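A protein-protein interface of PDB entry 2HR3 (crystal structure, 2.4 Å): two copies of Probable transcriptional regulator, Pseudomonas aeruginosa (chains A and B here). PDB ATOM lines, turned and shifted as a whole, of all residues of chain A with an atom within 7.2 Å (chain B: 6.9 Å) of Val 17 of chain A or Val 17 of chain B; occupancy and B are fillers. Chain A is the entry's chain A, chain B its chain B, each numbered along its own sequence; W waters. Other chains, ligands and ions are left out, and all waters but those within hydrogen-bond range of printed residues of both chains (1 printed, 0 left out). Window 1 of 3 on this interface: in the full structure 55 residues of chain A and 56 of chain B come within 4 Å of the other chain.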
ATOM      1  N   ALA A  11     -11.362  -4.572  -6.072  1.00  0.00           N
ATOM      2  CA  ALA A  11     -11.829  -5.623  -7.001  1.00  0.00           C
ATOM      3  C   ALA A  11     -12.349  -6.879  -6.299  1.00  0.00           C
ATOM      4  O   ALA A  11     -13.435  -7.359  -6.561  1.00  0.00           O
ATOM      5  CB  ALA A  11     -10.651  -6.034  -7.892  1.00  0.00           C
ATOM      6  N   HIS A  12     -11.563  -7.392  -5.367  1.00  0.00           N
ATOM      7  CA  HIS A  12     -11.985  -8.494  -4.519  1.00  0.00           C
ATOM      8  C   HIS A  12     -13.215  -8.228  -3.667  1.00  0.00           C
ATOM      9  O   HIS A  12     -14.160  -8.981  -3.692  1.00  0.00           O
ATOM     10  CB  HIS A  12     -10.830  -8.867  -3.607  1.00  0.00           C
ATOM     11  CG  HIS A  12      -9.682  -9.432  -4.345  1.00  0.00           C
ATOM     12  ND1 HIS A  12      -8.389  -9.319  -3.904  1.00  0.00           N
ATOM     13  CD2 HIS A  12      -9.632 -10.102  -5.517  1.00  0.00           C
ATOM     14  CE1 HIS A  12      -7.585  -9.929  -4.753  1.00  0.00           C
ATOM     15  NE2 HIS A  12      -8.315 -10.394  -5.754  1.00  0.00           N
ATOM     16  N   LEU A  13     -13.166  -7.172  -2.872  1.00  0.00           N
ATOM     17  CA  LEU A  13     -14.304  -6.784  -2.064  1.00  0.00           C
ATOM     18  C   LEU A  13     -15.546  -6.636  -2.917  1.00  0.00           C
ATOM     19  O   LEU A  13     -16.588  -7.190  -2.580  1.00  0.00           O
ATOM     20  CB  LEU A  13     -14.023  -5.507  -1.282  1.00  0.00           C
ATOM     21  CG  LEU A  13     -15.167  -5.026  -0.400  1.00  0.00           C
ATOM     22  CD1 LEU A  13     -15.686  -6.127   0.489  1.00  0.00           C
ATOM     23  CD2 LEU A  13     -14.714  -3.950   0.413  1.00  0.00           C
ATOM     24  N   ARG A  14     -15.467  -5.881  -4.016  1.00  0.00           N
ATOM     25  CA  ARG A  14     -16.583  -5.812  -4.983  1.00  0.00           C
ATOM     26  C   ARG A  14     -17.134  -7.203  -5.416  1.00  0.00           C
ATOM     27  O   ARG A  14     -18.336  -7.433  -5.447  1.00  0.00           O
ATOM     28  CB  ARG A  14     -16.130  -5.074  -6.254  1.00  0.00           C
ATOM     29  CG  ARG A  14     -17.333  -4.810  -7.270  1.00  0.00           C
ATOM     30  CD  ARG A  14     -16.920  -4.305  -8.656  1.00  0.00           C
ATOM     31  NE  ARG A  14     -15.809  -5.044  -9.266  1.00  0.00           N
ATOM     32  CZ  ARG A  14     -15.921  -6.283  -9.764  1.00  0.00           C
ATOM     33  NH1 ARG A  14     -17.035  -6.959  -9.692  1.00  0.00           N
ATOM     34  NH2 ARG A  14     -14.886  -6.887 -10.300  1.00  0.00           N
ATOM     35  N   SER A  15     -16.261  -8.125  -5.792  1.00  0.00           N
ATOM     36  CA  SER A  15     -16.770  -9.369  -6.377  1.00  0.00           C
ATOM     37  C   SER A  15     -17.401 -10.187  -5.278  1.00  0.00           C
ATOM     38  O   SER A  15     -18.485 -10.674  -5.453  1.00  0.00           O
ATOM     39  CB  SER A  15     -15.712 -10.170  -7.170  1.00  0.00           C
ATOM     40  OG  SER A  15     -14.727 -10.671  -6.283  1.00  0.00           O
ATOM     41  N   GLN A  16     -16.801 -10.170  -4.112  1.00  0.00           N
ATOM     42  CA  GLN A  16     -17.306 -10.904  -2.960  1.00  0.00           C
ATOM     43  C   GLN A  16     -18.672 -10.518  -2.455  1.00  0.00           C
ATOM     44  O   GLN A  16     -19.389 -11.351  -1.929  1.00  0.00           O
ATOM     45  CB  GLN A  16     -16.356 -10.693  -1.826  1.00  0.00           C
ATOM     46  CG  GLN A  16     -15.023 -11.357  -2.074  1.00  0.00           C
ATOM     47  CD  GLN A  16     -13.841 -10.721  -1.326  1.00  0.00           C
ATOM     48  OE1 GLN A  16     -13.969  -9.720  -0.603  1.00  0.00           O
ATOM     49  NE2 GLN A  16     -12.704 -11.335  -1.471  1.00  0.00           N
ATOM     50  N   VAL A  17     -18.929  -9.218  -2.446  1.00  0.00           N
ATOM     51  CA  VAL A  17     -20.087  -8.632  -1.832  1.00  0.00           C
ATOM     52  C   VAL A  17     -21.177  -8.752  -2.883  1.00  0.00           C
ATOM     53  O   VAL A  17     -22.300  -8.971  -2.545  1.00  0.00           O
ATOM     54  CB  VAL A  17     -19.804  -7.140  -1.431  1.00  0.00           C
ATOM     55  CG1 VAL A  17     -20.984  -6.323  -1.524  1.00  0.00           C
ATOM     56  CG2 VAL A  17     -19.262  -7.018  -0.033  1.00  0.00           C
ATOM     57  N   THR A  18     -20.847  -8.647  -4.170  1.00  0.00           N
ATOM     58  CA  THR A  18     -21.883  -8.744  -5.228  1.00  0.00           C
ATOM     59  C   THR A  18     -22.239 -10.219  -5.460  1.00  0.00           C
ATOM     60  O   THR A  18     -23.388 -10.584  -5.547  1.00  0.00           O
ATOM     61  CB  THR A  18     -21.563  -7.978  -6.552  1.00  0.00           C
ATOM     62  OG1 THR A  18     -20.655  -8.698  -7.362  1.00  0.00           O
ATOM     63  CG2 THR A  18     -21.007  -6.539  -6.337  1.00  0.00           C
ATOM     64  N   THR A  19     -21.241 -11.053  -5.504  1.00  0.00           N
ATOM     65  CA  THR A  19     -21.455 -12.467  -5.518  1.00  0.00           C
ATOM     66  C   THR A  19     -22.259 -13.010  -4.339  1.00  0.00           C
ATOM     67  O   THR A  19     -23.153 -13.842  -4.591  1.00  0.00           O
ATOM     68  CB  THR A  19     -20.108 -13.190  -5.563  1.00  0.00           C
ATOM     69  OG1 THR A  19     -19.432 -12.795  -6.768  1.00  0.00           O
ATOM     70  CG2 THR A  19     -20.316 -14.698  -5.564  1.00  0.00           C
ATOM     71  N   LEU A  20     -21.968 -12.611  -3.091  1.00  0.00           N
ATOM     72  CA  LEU A  20     -22.820 -13.043  -2.015  1.00  0.00           C
ATOM     73  C   LEU A  20     -24.253 -12.513  -2.166  1.00  0.00           C
ATOM     74  O   LEU A  20     -25.195 -13.246  -1.914  1.00  0.00           O
ATOM     75  CB  LEU A  20     -22.244 -12.742  -0.640  1.00  0.00           C
ATOM     76  CG  LEU A  20     -23.002 -13.243   0.592  1.00  0.00           C
ATOM     77  CD1 LEU A  20     -23.280 -14.738   0.583  1.00  0.00           C
ATOM     78  CD2 LEU A  20     -22.343 -12.913   1.942  1.00  0.00           C
ATOM     79  N   THR A  21     -24.429 -11.230  -2.549  1.00  0.00           N
ATOM     80  CA  THR A  21     -25.766 -10.622  -2.800  1.00  0.00           C
ATOM     81  C   THR A  21     -26.630 -11.366  -3.885  1.00  0.00           C
ATOM     82  O   THR A  21     -27.864 -11.478  -3.786  1.00  0.00           O
ATOM     83  CB  THR A  21     -25.595  -9.133  -3.199  1.00  0.00           C
ATOM     84  OG1 THR A  21     -24.982  -8.409  -2.129  1.00  0.00           O
ATOM     85  CG2 THR A  21     -26.998  -8.434  -3.634  1.00  0.00           C
ATOM     86  N   ARG A  22     -25.975 -11.876  -4.904  1.00  0.00           N
ATOM     87  CA  ARG A  22     -26.645 -12.625  -5.988  1.00  0.00           C
ATOM     88  C   ARG A  22     -27.097 -14.084  -5.573  1.00  0.00           C
ATOM     89  O   ARG A  22     -28.149 -14.573  -6.009  1.00  0.00           O
ATOM     90  CB  ARG A  22     -25.697 -12.657  -7.196  1.00  0.00           C
ATOM     91  CG  ARG A  22     -26.313 -13.187  -8.470  1.00  0.00           C
ATOM     92  CD  ARG A  22     -25.518 -12.865  -9.769  1.00  0.00           C
ATOM     93  NE  ARG A  22     -24.846 -11.558  -9.686  1.00  0.00           N
ATOM     94  CZ  ARG A  22     -23.522 -11.396  -9.598  1.00  0.00           C
ATOM     95  NH1 ARG A  22     -22.671 -12.442  -9.567  1.00  0.00           N
ATOM     96  NH2 ARG A  22     -23.039 -10.164  -9.518  1.00  0.00           N
ATOM     97  N   LEU A  24     -27.887 -14.790  -2.328  1.00  0.00           N
ATOM     98  CA  LEU A  24     -29.034 -14.444  -1.495  1.00  0.00           C
ATOM     99  C   LEU A  24     -30.268 -14.155  -2.322  1.00  0.00           C
ATOM    100  O   LEU A  24     -31.399 -14.359  -1.842  1.00  0.00           O
ATOM    101  CB  LEU A  24     -28.732 -13.206  -0.673  1.00  0.00           C
ATOM    102  CG  LEU A  24     -27.821 -13.262   0.522  1.00  0.00           C
ATOM    103  CD1 LEU A  24     -27.327 -11.861   0.969  1.00  0.00           C
ATOM    104  CD2 LEU A  24     -28.510 -13.933   1.649  1.00  0.00           C
ATOM    105  N   LEU A 115     -28.676 -18.309   5.564  1.00  0.00           N
ATOM    106  CA  LEU A 115     -27.298 -17.772   5.822  1.00  0.00           C
ATOM    107  C   LEU A 115     -26.692 -18.288   7.069  1.00  0.00           C
ATOM    108  O   LEU A 115     -25.485 -18.507   7.125  1.00  0.00           O
ATOM    109  CB  LEU A 115     -27.326 -16.271   5.997  1.00  0.00           C
ATOM    110  CG  LEU A 115     -26.344 -15.435   5.184  1.00  0.00           C
ATOM    111  CD1 LEU A 115     -26.516 -13.958   5.677  1.00  0.00           C
ATOM    112  CD2 LEU A 115     -24.908 -15.891   5.228  1.00  0.00           C
ATOM    113  N   GLY A 135     -18.631  -6.553   9.011  1.00  0.00           N
ATOM    114  CA  GLY A 135     -19.881  -6.280   8.335  1.00  0.00           C
ATOM    115  C   GLY A 135     -20.291  -4.842   8.500  1.00  0.00           C
ATOM    116  O   GLY A 135     -20.644  -4.129   7.559  1.00  0.00           O
ATOM    117  N   LEU A 138     -18.931  -2.395   5.937  1.00  0.00           N
ATOM    118  CA  LEU A 138     -19.589  -2.426   4.628  1.00  0.00           C
ATOM    119  C   LEU A 138     -20.652  -1.335   4.570  1.00  0.00           C
ATOM    120  O   LEU A 138     -20.787  -0.629   3.558  1.00  0.00           O
ATOM    121  CB  LEU A 138     -20.162  -3.820   4.357  1.00  0.00           C
ATOM    122  CG  LEU A 138     -19.113  -5.031   4.427  1.00  0.00           C
ATOM    123  CD1 LEU A 138     -19.766  -6.310   4.056  1.00  0.00           C
ATOM    124  CD2 LEU A 138     -17.910  -4.805   3.519  1.00  0.00           C
ATOM    125  N   THR A 139     -21.359  -1.194   5.686  1.00  0.00           N
ATOM    126  CA  THR A 139     -22.310  -0.107   5.925  1.00  0.00           C
ATOM    127  C   THR A 139     -21.600   1.253   5.868  1.00  0.00           C
ATOM    128  O   THR A 139     -22.051   2.185   5.227  1.00  0.00           O
ATOM    129  CB  THR A 139     -22.945  -0.236   7.311  1.00  0.00           C
ATOM    130  OG1 THR A 139     -23.519  -1.539   7.490  1.00  0.00           O
ATOM    131  CG2 THR A 139     -24.035   0.914   7.571  1.00  0.00           C
ATOM    132  N   HIS B  12     -27.923  -8.862  10.122  1.00  0.00           N
ATOM    133  CA  HIS B  12     -26.978  -7.781   9.913  1.00  0.00           C
ATOM    134  C   HIS B  12     -26.161  -7.995   8.691  1.00  0.00           C
ATOM    135  O   HIS B  12     -26.125  -7.098   7.838  1.00  0.00           O
ATOM    136  CB  HIS B  12     -26.027  -7.652  11.069  1.00  0.00           C
ATOM    137  CG  HIS B  12     -26.572  -6.875  12.216  1.00  0.00           C
ATOM    138  ND1 HIS B  12     -27.511  -7.386  13.081  1.00  0.00           N
ATOM    139  CD2 HIS B  12     -26.286  -5.631  12.663  1.00  0.00           C
ATOM    140  CE1 HIS B  12     -27.764  -6.509  14.026  1.00  0.00           C
ATOM    141  NE2 HIS B  12     -27.039  -5.433  13.792  1.00  0.00           N
ATOM    142  N   LEU B  13     -25.544  -9.180   8.565  1.00  0.00           N
ATOM    143  CA  LEU B  13     -24.696  -9.482   7.430  1.00  0.00           C
ATOM    144  C   LEU B  13     -25.352  -9.366   6.081  1.00  0.00           C
ATOM    145  O   LEU B  13     -24.750  -8.875   5.145  1.00  0.00           O
ATOM    146  CB  LEU B  13     -24.072 -10.914   7.545  1.00  0.00           C
ATOM    147  CG  LEU B  13     -22.997 -11.285   6.495  1.00  0.00           C
ATOM    148  CD1 LEU B  13     -21.901 -10.211   6.339  1.00  0.00           C
ATOM    149  CD2 LEU B  13     -22.380 -12.579   6.791  1.00  0.00           C
ATOM    150  N   ARG B  14     -26.558  -9.882   5.954  1.00  0.00           N
ATOM    151  CA  ARG B  14     -27.318  -9.760   4.739  1.00  0.00           C
ATOM    152  C   ARG B  14     -27.515  -8.286   4.389  1.00  0.00           C
ATOM    153  O   ARG B  14     -27.413  -7.861   3.259  1.00  0.00           O
ATOM    154  CB  ARG B  14     -28.699 -10.381   4.978  1.00  0.00           C
ATOM    155  CG  ARG B  14     -29.647 -10.284   3.757  1.00  0.00           C
ATOM    156  CD  ARG B  14     -31.082 -10.696   4.064  1.00  0.00           C
ATOM    157  NE  ARG B  14     -31.652  -9.848   5.112  1.00  0.00           N
ATOM    158  CZ  ARG B  14     -32.111  -8.601   4.935  1.00  0.00           C
ATOM    159  NH1 ARG B  14     -32.115  -7.997   3.748  1.00  0.00           N
ATOM    160  NH2 ARG B  14     -32.557  -7.963   5.979  1.00  0.00           N
ATOM    161  N   SER B  15     -27.845  -7.504   5.378  1.00  0.00           N
ATOM    162  CA  SER B  15     -28.203  -6.164   5.104  1.00  0.00           C
ATOM    163  C   SER B  15     -26.968  -5.382   4.678  1.00  0.00           C
ATOM    164  O   SER B  15     -26.975  -4.641   3.702  1.00  0.00           O
ATOM    165  CB  SER B  15     -28.793  -5.593   6.363  1.00  0.00           C
ATOM    166  OG  SER B  15     -29.423  -4.422   6.008  1.00  0.00           O
ATOM    167  N   GLN B  16     -25.886  -5.600   5.420  1.00  0.00           N
ATOM    168  CA  GLN B  16     -24.584  -5.017   5.134  1.00  0.00           C
ATOM    169  C   GLN B  16     -24.103  -5.336   3.752  1.00  0.00           C
ATOM    170  O   GLN B  16     -23.603  -4.475   3.102  1.00  0.00           O
ATOM    171  CB  GLN B  16     -23.591  -5.559   6.137  1.00  0.00           C
ATOM    172  CG  GLN B  16     -23.797  -4.987   7.505  1.00  0.00           C
ATOM    173  CD  GLN B  16     -23.324  -5.916   8.585  1.00  0.00           C
ATOM    174  OE1 GLN B  16     -22.938  -7.099   8.346  1.00  0.00           O
ATOM    175  NE2 GLN B  16     -23.381  -5.422   9.797  1.00  0.00           N
ATOM    176  N   VAL B  17     -24.237  -6.579   3.277  1.00  0.00           N
ATOM    177  CA  VAL B  17     -23.718  -6.892   1.947  1.00  0.00           C
ATOM    178  C   VAL B  17     -24.552  -6.265   0.831  1.00  0.00           C
ATOM    179  O   VAL B  17     -24.009  -5.782  -0.157  1.00  0.00           O
ATOM    180  CB  VAL B  17     -23.450  -8.392   1.695  1.00  0.00           C
ATOM    181  CG1 VAL B  17     -22.513  -8.968   2.759  1.00  0.00           C
ATOM    182  CG2 VAL B  17     -24.715  -9.181   1.578  1.00  0.00           C
ATOM    183  N   THR B  18     -25.862  -6.332   0.980  1.00  0.00           N
ATOM    184  CA  THR B  18     -26.770  -5.957  -0.107  1.00  0.00           C
ATOM    185  C   THR B  18     -26.913  -4.480  -0.178  1.00  0.00           C
ATOM    186  O   THR B  18     -27.425  -4.028  -1.132  1.00  0.00           O
ATOM    187  CB  THR B  18     -28.223  -6.586  -0.032  1.00  0.00           C
ATOM    188  OG1 THR B  18     -28.878  -6.159   1.139  1.00  0.00           O
ATOM    189  CG2 THR B  18     -28.157  -8.084   0.021  1.00  0.00           C
ATOM    190  N   THR B  19     -26.531  -3.764   0.874  1.00  0.00           N
ATOM    191  CA  THR B  19     -26.544  -2.318   0.897  1.00  0.00           C
ATOM    192  C   THR B  19     -25.335  -1.776   0.144  1.00  0.00           C
ATOM    193  O   THR B  19     -25.444  -0.847  -0.668  1.00  0.00           O
ATOM    194  CB  THR B  19     -26.472  -1.863   2.308  1.00  0.00           C
ATOM    195  OG1 THR B  19     -27.576  -2.436   3.021  1.00  0.00           O
ATOM    196  CG2 THR B  19     -26.573  -0.354   2.393  1.00  0.00           C
ATOM    197  N   LEU B  20     -24.188  -2.400   0.355  1.00  0.00           N
ATOM    198  CA  LEU B  20     -22.986  -1.910  -0.255  1.00  0.00           C
ATOM    199  C   LEU B  20     -23.096  -2.265  -1.733  1.00  0.00           C
ATOM    200  O   LEU B  20     -22.686  -1.493  -2.547  1.00  0.00           O
ATOM    201  CB  LEU B  20     -21.708  -2.438   0.427  1.00  0.00           C
ATOM    202  CG  LEU B  20     -20.429  -2.117  -0.379  1.00  0.00           C
ATOM    203  CD1 LEU B  20     -20.144  -0.643  -0.481  1.00  0.00           C
ATOM    204  CD2 LEU B  20     -19.322  -2.795   0.215  1.00  0.00           C
ATOM    205  N   THR B  21     -23.681  -3.405  -2.074  1.00  0.00           N
ATOM    206  CA  THR B  21     -23.948  -3.745  -3.483  1.00  0.00           C
ATOM    207  C   THR B  21     -24.932  -2.783  -4.220  1.00  0.00           C
ATOM    208  O   THR B  21     -24.708  -2.498  -5.397  1.00  0.00           O
ATOM    209  CB  THR B  21     -24.421  -5.222  -3.647  1.00  0.00           C
ATOM    210  OG1 THR B  21     -23.448  -6.096  -3.048  1.00  0.00           O
ATOM    211  CG2 THR B  21     -24.532  -5.611  -5.144  1.00  0.00           C
ATOM    212  N   ARG B  22     -26.004  -2.353  -3.559  1.00  0.00           N
ATOM    213  CA  ARG B  22     -26.810  -1.204  -3.947  1.00  0.00           C
ATOM    214  C   ARG B  22     -25.980   0.085  -4.157  1.00  0.00           C
ATOM    215  O   ARG B  22     -25.990   0.649  -5.251  1.00  0.00           O
ATOM    216  CB  ARG B  22     -27.900  -0.955  -2.898  1.00  0.00           C
ATOM    217  CG  ARG B  22     -29.354  -1.400  -3.355  1.00  0.00           C
ATOM    218  CD  ARG B  22     -30.460  -1.082  -2.354  1.00  0.00           C
ATOM    219  NE  ARG B  22     -30.482  -2.084  -1.307  1.00  0.00           N
ATOM    220  CZ  ARG B  22     -30.270  -1.851  -0.010  1.00  0.00           C
ATOM    221  NH1 ARG B  22     -30.034  -0.614   0.469  1.00  0.00           N
ATOM    222  NH2 ARG B  22     -30.289  -2.892   0.841  1.00  0.00           N
ATOM    223  N   LEU B  24     -22.859   0.131  -4.741  1.00  0.00           N
ATOM    224  CA  LEU B  24     -21.975  -0.089  -5.883  1.00  0.00           C
ATOM    225  C   LEU B  24     -22.624   0.242  -7.244  1.00  0.00           C
ATOM    226  O   LEU B  24     -21.973   0.842  -8.092  1.00  0.00           O
ATOM    227  CB  LEU B  24     -21.373  -1.491  -5.902  1.00  0.00           C
ATOM    228  CG  LEU B  24     -20.263  -1.701  -4.878  1.00  0.00           C
ATOM    229  CD1 LEU B  24     -19.977  -3.219  -4.750  1.00  0.00           C
ATOM    230  CD2 LEU B  24     -19.018  -0.863  -5.235  1.00  0.00           C
ATOM    231  N   GLY B 135     -13.137 -10.855   3.730  1.00  0.00           N
ATOM    232  CA  GLY B 135     -13.722 -10.844   2.406  1.00  0.00           C
ATOM    233  C   GLY B 135     -13.975 -12.227   1.871  1.00  0.00           C
ATOM    234  O   GLY B 135     -15.086 -12.580   1.520  1.00  0.00           O
ATOM    235  N   LEU B 138     -16.932 -14.307   2.616  1.00  0.00           N
ATOM    236  CA  LEU B 138     -18.104 -13.944   1.861  1.00  0.00           C
ATOM    237  C   LEU B 138     -18.261 -14.810   0.609  1.00  0.00           C
ATOM    238  O   LEU B 138     -19.384 -15.186   0.219  1.00  0.00           O
ATOM    239  CB  LEU B 138     -18.069 -12.465   1.502  1.00  0.00           C
ATOM    240  CG  LEU B 138     -18.178 -11.461   2.673  1.00  0.00           C
ATOM    241  CD1 LEU B 138     -18.265 -10.126   2.081  1.00  0.00           C
ATOM    242  CD2 LEU B 138     -19.346 -11.685   3.593  1.00  0.00           C
ATOM    243  N   THR B 139     -17.133 -15.078  -0.044  1.00  0.00           N
ATOM    244  CA  THR B 139     -17.065 -15.974  -1.208  1.00  0.00           C
ATOM    245  C   THR B 139     -17.454 -17.440  -0.882  1.00  0.00           C
ATOM    246  O   THR B 139     -18.155 -18.120  -1.643  1.00  0.00           O
ATOM    247  CB  THR B 139     -15.640 -15.929  -1.759  1.00  0.00           C
ATOM    248  OG1 THR B 139     -15.355 -14.600  -2.193  1.00  0.00           O
ATOM    249  CG2 THR B 139     -15.428 -16.910  -2.975  1.00  0.00           C
HETATM  250  O   HOH W   1     -24.002  -2.286  10.093  1.00  0.00           O
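The side-chain hydroxyl (OG1) of Thr 21 of chain B sits at hydrogen-bond distance from the side-chain hydroxyl (OG1) of Thr 21 of chain A (2.9 Å).
The backbone carbonyl oxygen (O) of Val 17 of chain A lies close to the side-chain hydroxyl (OG1) of Thr 21 of chain B, at 3.1 Å.
The side-chain hydroxyl (OG1) of Thr 21 of chain A sits at hydrogen-bond distance from the backbone carbonyl oxygen (O) of Val 17 of chain B, at 3.4 Å.
OG1 of Thr 21 of chain A is in hydrogen-bond range of O of Val 17 of chain A, at 2.8 Å.
The side-chain hydroxyl (OG1) of Thr 21 of chain B sits at hydrogen-bond distance from the backbone carbonyl oxygen (O) of Val 17 of chain B.
O of His 12 of chain B lies close to OE1 of Gln 16 of chain B.
The backbone carbonyl oxygen (O) of Arg 14 of chain B lies within hydrogen-bond range of the side-chain hydroxyl (OG1) of Thr 18 of chain B (3.1 Å).
The side-chain amide oxygen (OE1) of Gln 16 of chain B lies close to the backbone NH (N) of Leu 13 of chain B (3.3 Å).
The backbone carbonyl oxygen (O) of Arg 14 of chain A lies close to the side-chain hydroxyl (OG1) of Thr 18 of chain A (3.3 Å).
Among the printed residues, pairs that only touch across the chains: Arg 14 of chain A with Leu 24 of chain B (3.98 Å), Gln 16 of chain A with Gly 135 of chain B (3.2 Å), Gln 16 of chain A with Leu 138 of chain B (3.8 Å), Gln 16 of chain A with Thr 139 of chain B (3.3 Å), Val 17 of chain A with Val 17 of chain B (3.4 Å), Val 17 of chain A with Leu 138 of chain B (3.9 Å), Thr 18 of chain A with Thr 21 of chain B (3.8 Å), Thr 18 of chain A with Leu 24 of chain B (3.8 Å), Leu 20 of chain A with Leu 138 of chain B (3.6 Å), Thr 21 of chain A with Thr 18 of chain B (3.6 Å), Leu 24 of chain A with Arg 14 of chain B (3.96 Å), Leu 24 of chain A with Val 17 of chain B (3.8 Å), Leu 24 of chain A with Thr 18 of chain B (3.98 Å), Gly 135 of chain A with Gln 16 of chain B (3.2 Å), Leu 138 of chain A with Gln 16 of chain B (3.7 Å), Leu 138 of chain A with Leu 20 of chain B (3.7 Å) and Thr 139 of chain A with Gln 16 of chain B (3.5 Å).
Val 17 of chain B touches just these residues of chain A: Val 17, Thr 21 and Leu 24.
Of the printed residues of chain A, Thr 18 of chain B touches Thr 21 (3.6 Å) and Leu 24 (3.98 Å).
Of the printed residues of chain B, Leu 24 of chain A touches Arg 14 (3.96 Å), Val 17 (3.8 Å) and Thr 18 (3.98 Å).
Of the printed residues of chain B, Thr 139 of chain A touches Gln 16 (3.5 Å).
Of the printed residues of chain B, Gln 16 of chain A touches Gly 135, Leu 138 and Thr 139.
Of the 15 printed residues of chain B, 10 touch a printed residue of chain A.
Printed residues of chain B that touch a printed residue of chain A: Arg 14, Gln 16, Val 17, Thr 18, Leu 20, Thr 21, Leu 24, Gly 135, Leu 138 and Thr 139.
Hydrophobic or aromatic side chains of chain B within 4 Å of the printed part of chain A: Val 17, Leu 20, Leu 24 and Leu 138.
Along chain A the printed residues that touch a printed residue of chain B span positions 14 to 139.
Among the printed residues, no Asp or Glu carboxylate lies within 4 Å of a Lys or Arg side-chain nitrogen of the other chain.
Arg 14 of chain A touches Leu 24 of chain B, and with the chains exchanged Leu 24 of chain A touches Arg 14 of chain B.
Val 17 of chain A touches Thr 21 of chain B, and with the chains exchanged Thr 21 of chain A touches Val 17 of chain B.
Thr 18 of chain A touches Thr 21 of chain B, and with the chains exchanged Thr 21 of chain A touches Thr 18 of chain B.
Leu 20 of chain A touches Leu 138 of chain B, and with the chains exchanged Leu 138 of chain A touches Leu 20 of chain B.
Positions printed for both chains: 12, 13, 14, 15, 16, 17, 18, 19, 20, 21, 22, 24, 135, 138 and 139.
Of the 20 pairs that touch across the chains among the printed residues, 18 have their exchanged pair printed and touching as well.
Water W1 lies within hydrogen-bond range of OG1 of Thr 139 of chain A (2.8 Å) and NE2 of Gln 16 of chain B (3.2 Å).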
